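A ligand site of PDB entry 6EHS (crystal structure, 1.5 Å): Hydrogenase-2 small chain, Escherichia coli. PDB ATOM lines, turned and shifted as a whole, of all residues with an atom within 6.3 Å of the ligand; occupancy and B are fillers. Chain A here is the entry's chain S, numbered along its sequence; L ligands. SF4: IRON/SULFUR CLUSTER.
A ring nitrogen (ND1) of His 193 is bound to an iron atom (FE3) of the ligand (2.1 Å). The side-chain sulfur of Cys 196 binds an iron atom (FE4) of the ligand, 2.3 Å away. SG of Cys 221 binds FE1 of the ligand (2.3 Å). An iron atom (FE2) of the ligand is bound by the side-chain sulfur (SG) of Cys 227 (2.3 Å). The backbone NH (N) of Arg 199 sits close to a sulfur (S2) of the ligand. The backbone NH (N) of Leu 222 sits close to a sulfur (S3) of the ligand, 3.5 Å away.
Arg 198 touches the ligand (C to S2, 3.6 Å). Phe 202 touches the ligand. Tyr 223 touches the ligand. Gly 229 touches the ligand (CA to S1, 3.7 Å). Pro 230 touches the ligand. Val 250 touches the ligand. 12 residues have an atom within 4 Å of the ligand: His 193, Cys 196, Arg 198, Arg 199, Phe 202, Cys 221, Leu 222, Tyr 223, Cys 227, Gly 229, Pro 230 and Val 250. The nearest printed residue that does not touch the ligand is Ile 192 (4.1 Å).
The guanidinium group (NH1) of Arg 199 lies within hydrogen-bond range of the backbone carbonyl oxygen (O) of His 193 (3.3 Å). SG of Cys 196 lies close to N of Arg 198 (3.3 Å). SG of Cys 221 sits close to N of Tyr 223 (3.3 Å). The backbone NH of Cys 227 sits at hydrogen-bond distance from the backbone carbonyl oxygen of Leu 222, at 3.3 Å. SG of Cys 227 sits close to N of Gly 229 (3.5 Å). OE1 of Glu 194 lies within salt-bridge range of NH1 of Arg 199 (3.0 Å). O of Val 250 is in hydrogen-bond range of NH2 of Arg 198 (3.2 Å). The backbone carbonyl oxygen (O) of Trp 220 is in hydrogen-bond range of the guanidinium group (NH1) of Arg 198 (2.9 Å).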
ATOM      1  N   ILE A 192      26.001 -10.890   8.369  1.00  0.00           N
ATOM      2  CA  ILE A 192      26.931 -11.173   9.443  1.00  0.00           C
ATOM      3  C   ILE A 192      26.134 -11.654  10.669  1.00  0.00           C
ATOM      4  O   ILE A 192      26.522 -12.648  11.305  1.00  0.00           O
ATOM      5  CB  ILE A 192      27.852  -9.971   9.718  1.00  0.00           C
ATOM      6  CG1 ILE A 192      28.847  -9.827   8.543  1.00  0.00           C
ATOM      7  CG2 ILE A 192      28.583 -10.143  11.038  1.00  0.00           C
ATOM      8  CD1 ILE A 192      29.568  -8.487   8.540  1.00  0.00           C
ATOM      9  N   HIS A 193      25.043 -10.969  11.005  1.00  0.00           N
ATOM     10  CA  HIS A 193      24.199 -11.336  12.157  1.00  0.00           C
ATOM     11  C   HIS A 193      23.539 -12.709  12.033  1.00  0.00           C
ATOM     12  O   HIS A 193      23.108 -13.260  13.036  1.00  0.00           O
ATOM     13  CB  HIS A 193      23.138 -10.250  12.290  1.00  0.00           C
ATOM     14  CG  HIS A 193      22.208 -10.347  13.436  1.00  0.00           C
ATOM     15  ND1 HIS A 193      22.557 -10.038  14.740  1.00  0.00           N
ATOM     16  CD2 HIS A 193      20.887 -10.672  13.458  1.00  0.00           C
ATOM     17  CE1 HIS A 193      21.496 -10.194  15.508  1.00  0.00           C
ATOM     18  NE2 HIS A 193      20.460 -10.571  14.754  1.00  0.00           N
ATOM     19  N   GLU A 194      23.421 -13.216  10.820  1.00  0.00           N
ATOM     20  CA  GLU A 194      22.865 -14.549  10.612  1.00  0.00           C
ATOM     21  C   GLU A 194      23.944 -15.643  10.672  1.00  0.00           C
ATOM     22  O   GLU A 194      23.668 -16.818  10.378  1.00  0.00           O
ATOM     23  CB  GLU A 194      22.036 -14.623   9.342  1.00  0.00           C
ATOM     24  CG  GLU A 194      20.758 -13.789   9.448  1.00  0.00           C
ATOM     25  CD  GLU A 194      19.839 -14.147  10.630  1.00  0.00           C
ATOM     26  OE1 GLU A 194      19.398 -13.271  11.428  1.00  0.00           O
ATOM     27  OE2 GLU A 194      19.546 -15.322  10.797  1.00  0.00           O
ATOM     28  N   CYS A 196      26.759 -15.030  13.334  1.00  0.00           N
ATOM     29  CA  CYS A 196      27.619 -14.373  14.341  1.00  0.00           C
ATOM     30  C   CYS A 196      27.582 -15.148  15.639  1.00  0.00           C
ATOM     31  O   CYS A 196      26.482 -15.454  16.156  1.00  0.00           O
ATOM     32  CB  CYS A 196      27.098 -12.947  14.628  1.00  0.00           C
ATOM     33  SG  CYS A 196      28.123 -12.094  15.907  1.00  0.00           S
ATOM     34  N   GLU A 197      28.778 -15.418  16.186  1.00  0.00           N
ATOM     35  CA  GLU A 197      28.911 -16.151  17.414  1.00  0.00           C
ATOM     36  C   GLU A 197      28.385 -15.431  18.638  1.00  0.00           C
ATOM     37  O   GLU A 197      28.230 -16.084  19.709  1.00  0.00           O
ATOM     38  CB  GLU A 197      30.377 -16.582  17.603  1.00  0.00           C
ATOM     39  CG  GLU A 197      31.343 -15.461  17.924  1.00  0.00           C
ATOM     40  CD  GLU A 197      31.973 -14.732  16.725  1.00  0.00           C
ATOM     41  OE1 GLU A 197      31.450 -14.832  15.548  1.00  0.00           O
ATOM     42  OE2 GLU A 197      33.003 -14.023  17.011  1.00  0.00           O
ATOM     43  N   ARG A 198      28.052 -14.128  18.539  1.00  0.00           N
ATOM     44  CA  ARG A 198      27.459 -13.468  19.696  1.00  0.00           C
ATOM     45  C   ARG A 198      25.928 -13.468  19.619  1.00  0.00           C
ATOM     46  O   ARG A 198      25.253 -12.927  20.537  1.00  0.00           O
ATOM     47  CB  ARG A 198      27.972 -12.040  19.861  1.00  0.00           C
ATOM     48  CG  ARG A 198      29.497 -12.072  19.988  1.00  0.00           C
ATOM     49  CD  ARG A 198      30.085 -10.805  20.455  1.00  0.00           C
ATOM     50  NE  ARG A 198      31.511 -10.983  20.677  1.00  0.00           N
ATOM     51  CZ  ARG A 198      32.262 -10.212  21.414  1.00  0.00           C
ATOM     52  NH1 ARG A 198      31.771  -9.103  21.973  1.00  0.00           N
ATOM     53  NH2 ARG A 198      33.564 -10.512  21.501  1.00  0.00           N
ATOM     54  N   ARG A 199      25.357 -14.137  18.613  1.00  0.00           N
ATOM     55  CA  ARG A 199      23.899 -14.214  18.505  1.00  0.00           C
ATOM     56  C   ARG A 199      23.199 -14.781  19.776  1.00  0.00           C
ATOM     57  O   ARG A 199      22.084 -14.306  20.134  1.00  0.00           O
ATOM     58  CB  ARG A 199      23.485 -15.016  17.274  1.00  0.00           C
ATOM     59  CG  ARG A 199      21.963 -15.102  17.065  1.00  0.00           C
ATOM     60  CD  ARG A 199      21.255 -13.725  16.893  1.00  0.00           C
ATOM     61  NE  ARG A 199      19.888 -14.039  16.537  1.00  0.00           N
ATOM     62  CZ  ARG A 199      19.420 -14.226  15.303  1.00  0.00           C
ATOM     63  NH1 ARG A 199      20.153 -13.980  14.227  1.00  0.00           N
ATOM     64  NH2 ARG A 199      18.167 -14.663  15.152  1.00  0.00           N
ATOM     65  N   PRO A 200      23.790 -15.777  20.444  1.00  0.00           N
ATOM     66  CA  PRO A 200      23.118 -16.176  21.698  1.00  0.00           C
ATOM     67  C   PRO A 200      22.928 -15.057  22.744  1.00  0.00           C
ATOM     68  O   PRO A 200      21.944 -15.050  23.494  1.00  0.00           O
ATOM     69  CB  PRO A 200      24.054 -17.262  22.261  1.00  0.00           C
ATOM     70  CG  PRO A 200      24.804 -17.769  21.079  1.00  0.00           C
ATOM     71  CD  PRO A 200      24.985 -16.595  20.173  1.00  0.00           C
ATOM     72  N   PHE A 202      22.705 -11.759  21.976  1.00  0.00           N
ATOM     73  CA  PHE A 202      21.616 -10.973  21.389  1.00  0.00           C
ATOM     74  C   PHE A 202      20.252 -11.584  21.805  1.00  0.00           C
ATOM     75  O   PHE A 202      19.367 -10.870  22.306  1.00  0.00           O
ATOM     76  CB  PHE A 202      21.758 -10.942  19.855  1.00  0.00           C
ATOM     77  CG  PHE A 202      20.676 -10.156  19.153  1.00  0.00           C
ATOM     78  CD1 PHE A 202      19.492 -10.759  18.784  1.00  0.00           C
ATOM     79  CD2 PHE A 202      20.860  -8.828  18.823  1.00  0.00           C
ATOM     80  CE1 PHE A 202      18.495 -10.052  18.162  1.00  0.00           C
ATOM     81  CE2 PHE A 202      19.871  -8.109  18.181  1.00  0.00           C
ATOM     82  CZ  PHE A 202      18.694  -8.718  17.847  1.00  0.00           C
ATOM     83  N   PHE A 207      23.806  -7.615  26.462  1.00  0.00           N
ATOM     84  CA  PHE A 207      24.439  -6.585  25.660  1.00  0.00           C
ATOM     85  C   PHE A 207      25.501  -5.826  26.402  1.00  0.00           C
ATOM     86  O   PHE A 207      25.313  -5.445  27.557  1.00  0.00           O
ATOM     87  CB  PHE A 207      23.370  -5.571  25.271  1.00  0.00           C
ATOM     88  CG  PHE A 207      22.271  -6.140  24.430  1.00  0.00           C
ATOM     89  CD1 PHE A 207      22.546  -6.609  23.176  1.00  0.00           C
ATOM     90  CD2 PHE A 207      20.965  -6.194  24.881  1.00  0.00           C
ATOM     91  CE1 PHE A 207      21.557  -7.104  22.348  1.00  0.00           C
ATOM     92  CE2 PHE A 207      19.968  -6.692  24.068  1.00  0.00           C
ATOM     93  CZ  PHE A 207      20.252  -7.149  22.795  1.00  0.00           C
ATOM     94  N   TRP A 220      29.862 -10.072  25.258  1.00  0.00           N
ATOM     95  CA  TRP A 220      28.444 -10.045  24.954  1.00  0.00           C
ATOM     96  C   TRP A 220      28.177  -9.345  23.610  1.00  0.00           C
ATOM     97  O   TRP A 220      29.093  -8.795  22.989  1.00  0.00           O
ATOM     98  CB  TRP A 220      27.685  -9.377  26.100  1.00  0.00           C
ATOM     99  CG  TRP A 220      27.524 -10.234  27.322  1.00  0.00           C
ATOM    100  CD1 TRP A 220      28.019 -11.486  27.510  1.00  0.00           C
ATOM    101  CD2 TRP A 220      26.807  -9.901  28.517  1.00  0.00           C
ATOM    102  NE1 TRP A 220      27.666 -11.948  28.757  1.00  0.00           N
ATOM    103  CE2 TRP A 220      26.924 -10.993  29.390  1.00  0.00           C
ATOM    104  CE3 TRP A 220      26.089  -8.781  28.921  1.00  0.00           C
ATOM    105  CZ2 TRP A 220      26.311 -11.017  30.649  1.00  0.00           C
ATOM    106  CZ3 TRP A 220      25.475  -8.804  30.179  1.00  0.00           C
ATOM    107  CH2 TRP A 220      25.620  -9.897  31.034  1.00  0.00           C
ATOM    108  N   CYS A 221      26.935  -9.381  23.159  1.00  0.00           N
ATOM    109  CA  CYS A 221      26.565  -8.817  21.838  1.00  0.00           C
ATOM    110  C   CYS A 221      26.762  -7.294  21.848  1.00  0.00           C
ATOM    111  O   CYS A 221      26.559  -6.627  22.877  1.00  0.00           O
ATOM    112  CB  CYS A 221      25.097  -9.177  21.532  1.00  0.00           C
ATOM    113  SG  CYS A 221      24.359  -8.304  20.167  1.00  0.00           S
ATOM    114  N   LEU A 222      27.204  -6.803  20.699  1.00  0.00           N
ATOM    115  CA  LEU A 222      27.482  -5.388  20.495  1.00  0.00           C
ATOM    116  C   LEU A 222      26.387  -4.572  19.806  1.00  0.00           C
ATOM    117  O   LEU A 222      26.603  -3.413  19.385  1.00  0.00           O
ATOM    118  CB  LEU A 222      28.803  -5.262  19.756  1.00  0.00           C
ATOM    119  CG  LEU A 222      29.975  -6.087  20.325  1.00  0.00           C
ATOM    120  CD1 LEU A 222      31.291  -5.810  19.576  1.00  0.00           C
ATOM    121  CD2 LEU A 222      30.151  -5.807  21.818  1.00  0.00           C
ATOM    122  N   TYR A 223      25.189  -5.134  19.729  1.00  0.00           N
ATOM    123  CA  TYR A 223      24.048  -4.473  19.056  1.00  0.00           C
ATOM    124  C   TYR A 223      23.825  -3.049  19.575  1.00  0.00           C
ATOM    125  O   TYR A 223      23.710  -2.094  18.786  1.00  0.00           O
ATOM    126  CB  TYR A 223      22.755  -5.291  19.193  1.00  0.00           C
ATOM    127  CG  TYR A 223      21.587  -4.608  18.517  1.00  0.00           C
ATOM    128  CD1 TYR A 223      21.504  -4.555  17.129  1.00  0.00           C
ATOM    129  CD2 TYR A 223      20.627  -3.950  19.259  1.00  0.00           C
ATOM    130  CE1 TYR A 223      20.501  -3.866  16.494  1.00  0.00           C
ATOM    131  CE2 TYR A 223      19.622  -3.247  18.652  1.00  0.00           C
ATOM    132  CZ  TYR A 223      19.554  -3.219  17.260  1.00  0.00           C
ATOM    133  OH  TYR A 223      18.549  -2.493  16.631  1.00  0.00           O
ATOM    134  N   HIS A 224      23.807  -2.892  20.895  1.00  0.00           N
ATOM    135  CA  HIS A 224      23.531  -1.576  21.502  1.00  0.00           C
ATOM    136  C   HIS A 224      24.702  -0.609  21.447  1.00  0.00           C
ATOM    137  O   HIS A 224      24.536   0.537  21.836  1.00  0.00           O
ATOM    138  CB  HIS A 224      22.903  -1.730  22.904  1.00  0.00           C
ATOM    139  CG  HIS A 224      21.443  -2.048  22.850  1.00  0.00           C
ATOM    140  ND1 HIS A 224      20.497  -1.098  22.557  1.00  0.00           N
ATOM    141  CD2 HIS A 224      20.780  -3.218  22.986  1.00  0.00           C
ATOM    142  CE1 HIS A 224      19.297  -1.669  22.530  1.00  0.00           C
ATOM    143  NE2 HIS A 224      19.443  -2.966  22.772  1.00  0.00           N
ATOM    144  N   CYS A 227      26.272  -2.112  16.409  1.00  0.00           N
ATOM    145  CA  CYS A 227      26.673  -3.139  15.452  1.00  0.00           C
ATOM    146  C   CYS A 227      25.758  -3.189  14.241  1.00  0.00           C
ATOM    147  O   CYS A 227      24.541  -3.293  14.371  1.00  0.00           O
ATOM    148  CB  CYS A 227      26.741  -4.470  16.142  1.00  0.00           C
ATOM    149  SG  CYS A 227      27.435  -5.800  15.113  1.00  0.00           S
ATOM    150  N   LYS A 228      26.384  -3.136  13.067  1.00  0.00           N
ATOM    151  CA  LYS A 228      25.671  -3.214  11.810  1.00  0.00           C
ATOM    152  C   LYS A 228      25.563  -4.604  11.213  1.00  0.00           C
ATOM    153  O   LYS A 228      25.095  -4.796  10.084  1.00  0.00           O
ATOM    154  CB  LYS A 228      26.243  -2.198  10.827  1.00  0.00           C
ATOM    155  CG  LYS A 228      26.258  -0.749  11.322  1.00  0.00           C
ATOM    156  CD  LYS A 228      24.888  -0.288  11.863  1.00  0.00           C
ATOM    157  CE  LYS A 228      24.929   1.218  12.086  1.00  0.00           C
ATOM    158  NZ  LYS A 228      25.979   1.613  13.089  1.00  0.00           N
ATOM    159  N   GLY A 229      25.975  -5.599  11.968  1.00  0.00           N
ATOM    160  CA  GLY A 229      25.834  -6.994  11.519  1.00  0.00           C
ATOM    161  C   GLY A 229      24.465  -7.356  10.992  1.00  0.00           C
ATOM    162  O   GLY A 229      24.344  -8.086  10.007  1.00  0.00           O
ATOM    163  N   PRO A 230      23.415  -6.827  11.615  1.00  0.00           N
ATOM    164  CA  PRO A 230      22.039  -7.166  11.136  1.00  0.00           C
ATOM    165  C   PRO A 230      21.669  -6.683   9.739  1.00  0.00           C
ATOM    166  O   PRO A 230      20.677  -7.151   9.173  1.00  0.00           O
ATOM    167  CB  PRO A 230      21.134  -6.570  12.198  1.00  0.00           C
ATOM    168  CG  PRO A 230      21.982  -6.581  13.433  1.00  0.00           C
ATOM    169  CD  PRO A 230      23.362  -6.194  12.945  1.00  0.00           C
ATOM    170  N   TRP A 248      38.269 -10.519  14.069  1.00  0.00           N
ATOM    171  CA  TRP A 248      37.410  -9.619  13.294  1.00  0.00           C
ATOM    172  C   TRP A 248      36.947  -8.549  14.215  1.00  0.00           C
ATOM    173  O   TRP A 248      37.164  -8.638  15.433  1.00  0.00           O
ATOM    174  CB  TRP A 248      36.261 -10.394  12.642  1.00  0.00           C
ATOM    175  CG  TRP A 248      35.145 -11.004  13.496  1.00  0.00           C
ATOM    176  CD1 TRP A 248      35.222 -12.061  14.342  1.00  0.00           C
ATOM    177  CD2 TRP A 248      33.773 -10.615  13.446  1.00  0.00           C
ATOM    178  NE1 TRP A 248      33.971 -12.335  14.855  1.00  0.00           N
ATOM    179  CE2 TRP A 248      33.046 -11.488  14.307  1.00  0.00           C
ATOM    180  CE3 TRP A 248      33.065  -9.643  12.732  1.00  0.00           C
ATOM    181  CZ2 TRP A 248      31.668 -11.399  14.487  1.00  0.00           C
ATOM    182  CZ3 TRP A 248      31.710  -9.567  12.888  1.00  0.00           C
ATOM    183  CH2 TRP A 248      31.002 -10.453  13.749  1.00  0.00           C
ATOM    184  N   VAL A 250      34.170  -7.471  15.729  1.00  0.00           N
ATOM    185  CA  VAL A 250      33.291  -7.827  16.853  1.00  0.00           C
ATOM    186  C   VAL A 250      34.059  -8.698  17.811  1.00  0.00           C
ATOM    187  O   VAL A 250      33.983  -8.461  19.032  1.00  0.00           O
ATOM    188  CB  VAL A 250      32.012  -8.511  16.344  1.00  0.00           C
ATOM    189  CG1 VAL A 250      31.254  -9.216  17.456  1.00  0.00           C
ATOM    190  CG2 VAL A 250      31.098  -7.492  15.646  1.00  0.00           C
ATOM    191  N   PRO A 255      31.789  -2.930  17.457  1.00  0.00           N
ATOM    192  CA  PRO A 255      30.700  -3.246  16.543  1.00  0.00           C
ATOM    193  C   PRO A 255      31.138  -3.216  15.082  1.00  0.00           C
ATOM    194  O   PRO A 255      32.025  -2.463  14.696  1.00  0.00           O
ATOM    195  CB  PRO A 255      29.691  -2.121  16.790  1.00  0.00           C
ATOM    196  CG  PRO A 255      30.439  -1.068  17.513  1.00  0.00           C
ATOM    197  CD  PRO A 255      31.460  -1.775  18.300  1.00  0.00           C
ATOM    198  N   CYS A 256      30.487  -4.032  14.268  1.00  0.00           N
ATOM    199  CA  CYS A 256      30.517  -3.854  12.814  1.00  0.00           C
ATOM    200  C   CYS A 256      29.955  -2.448  12.473  1.00  0.00           C
ATOM    201  O   CYS A 256      28.944  -2.029  13.077  1.00  0.00           O
ATOM    202  CB  CYS A 256      29.717  -4.966  12.144  1.00  0.00           C
ATOM    203  SG  CYS A 256      29.499  -4.804  10.360  1.00  0.00           S
HETATM  204 FE1  SF4 L   1      25.235  -8.909  18.129  1.00  0.00          FE
HETATM  205 FE2  SF4 L   1      26.441  -7.701  15.941  1.00  0.00          FE
HETATM  206 FE3  SF4 L   1      24.328  -9.425  15.627  1.00  0.00          FE
HETATM  207 FE4  SF4 L   1      26.752 -10.349  16.364  1.00  0.00          FE
HETATM  208  S1  SF4 L   1      26.228  -9.310  14.337  1.00  0.00           S
HETATM  209  S2  SF4 L   1      24.729 -10.966  17.304  1.00  0.00           S
HETATM  210  S3  SF4 L   1      27.488  -8.698  17.750  1.00  0.00           S
HETATM  211  S4  SF4 L   1      24.256  -7.404  16.648  1.00  0.00           S
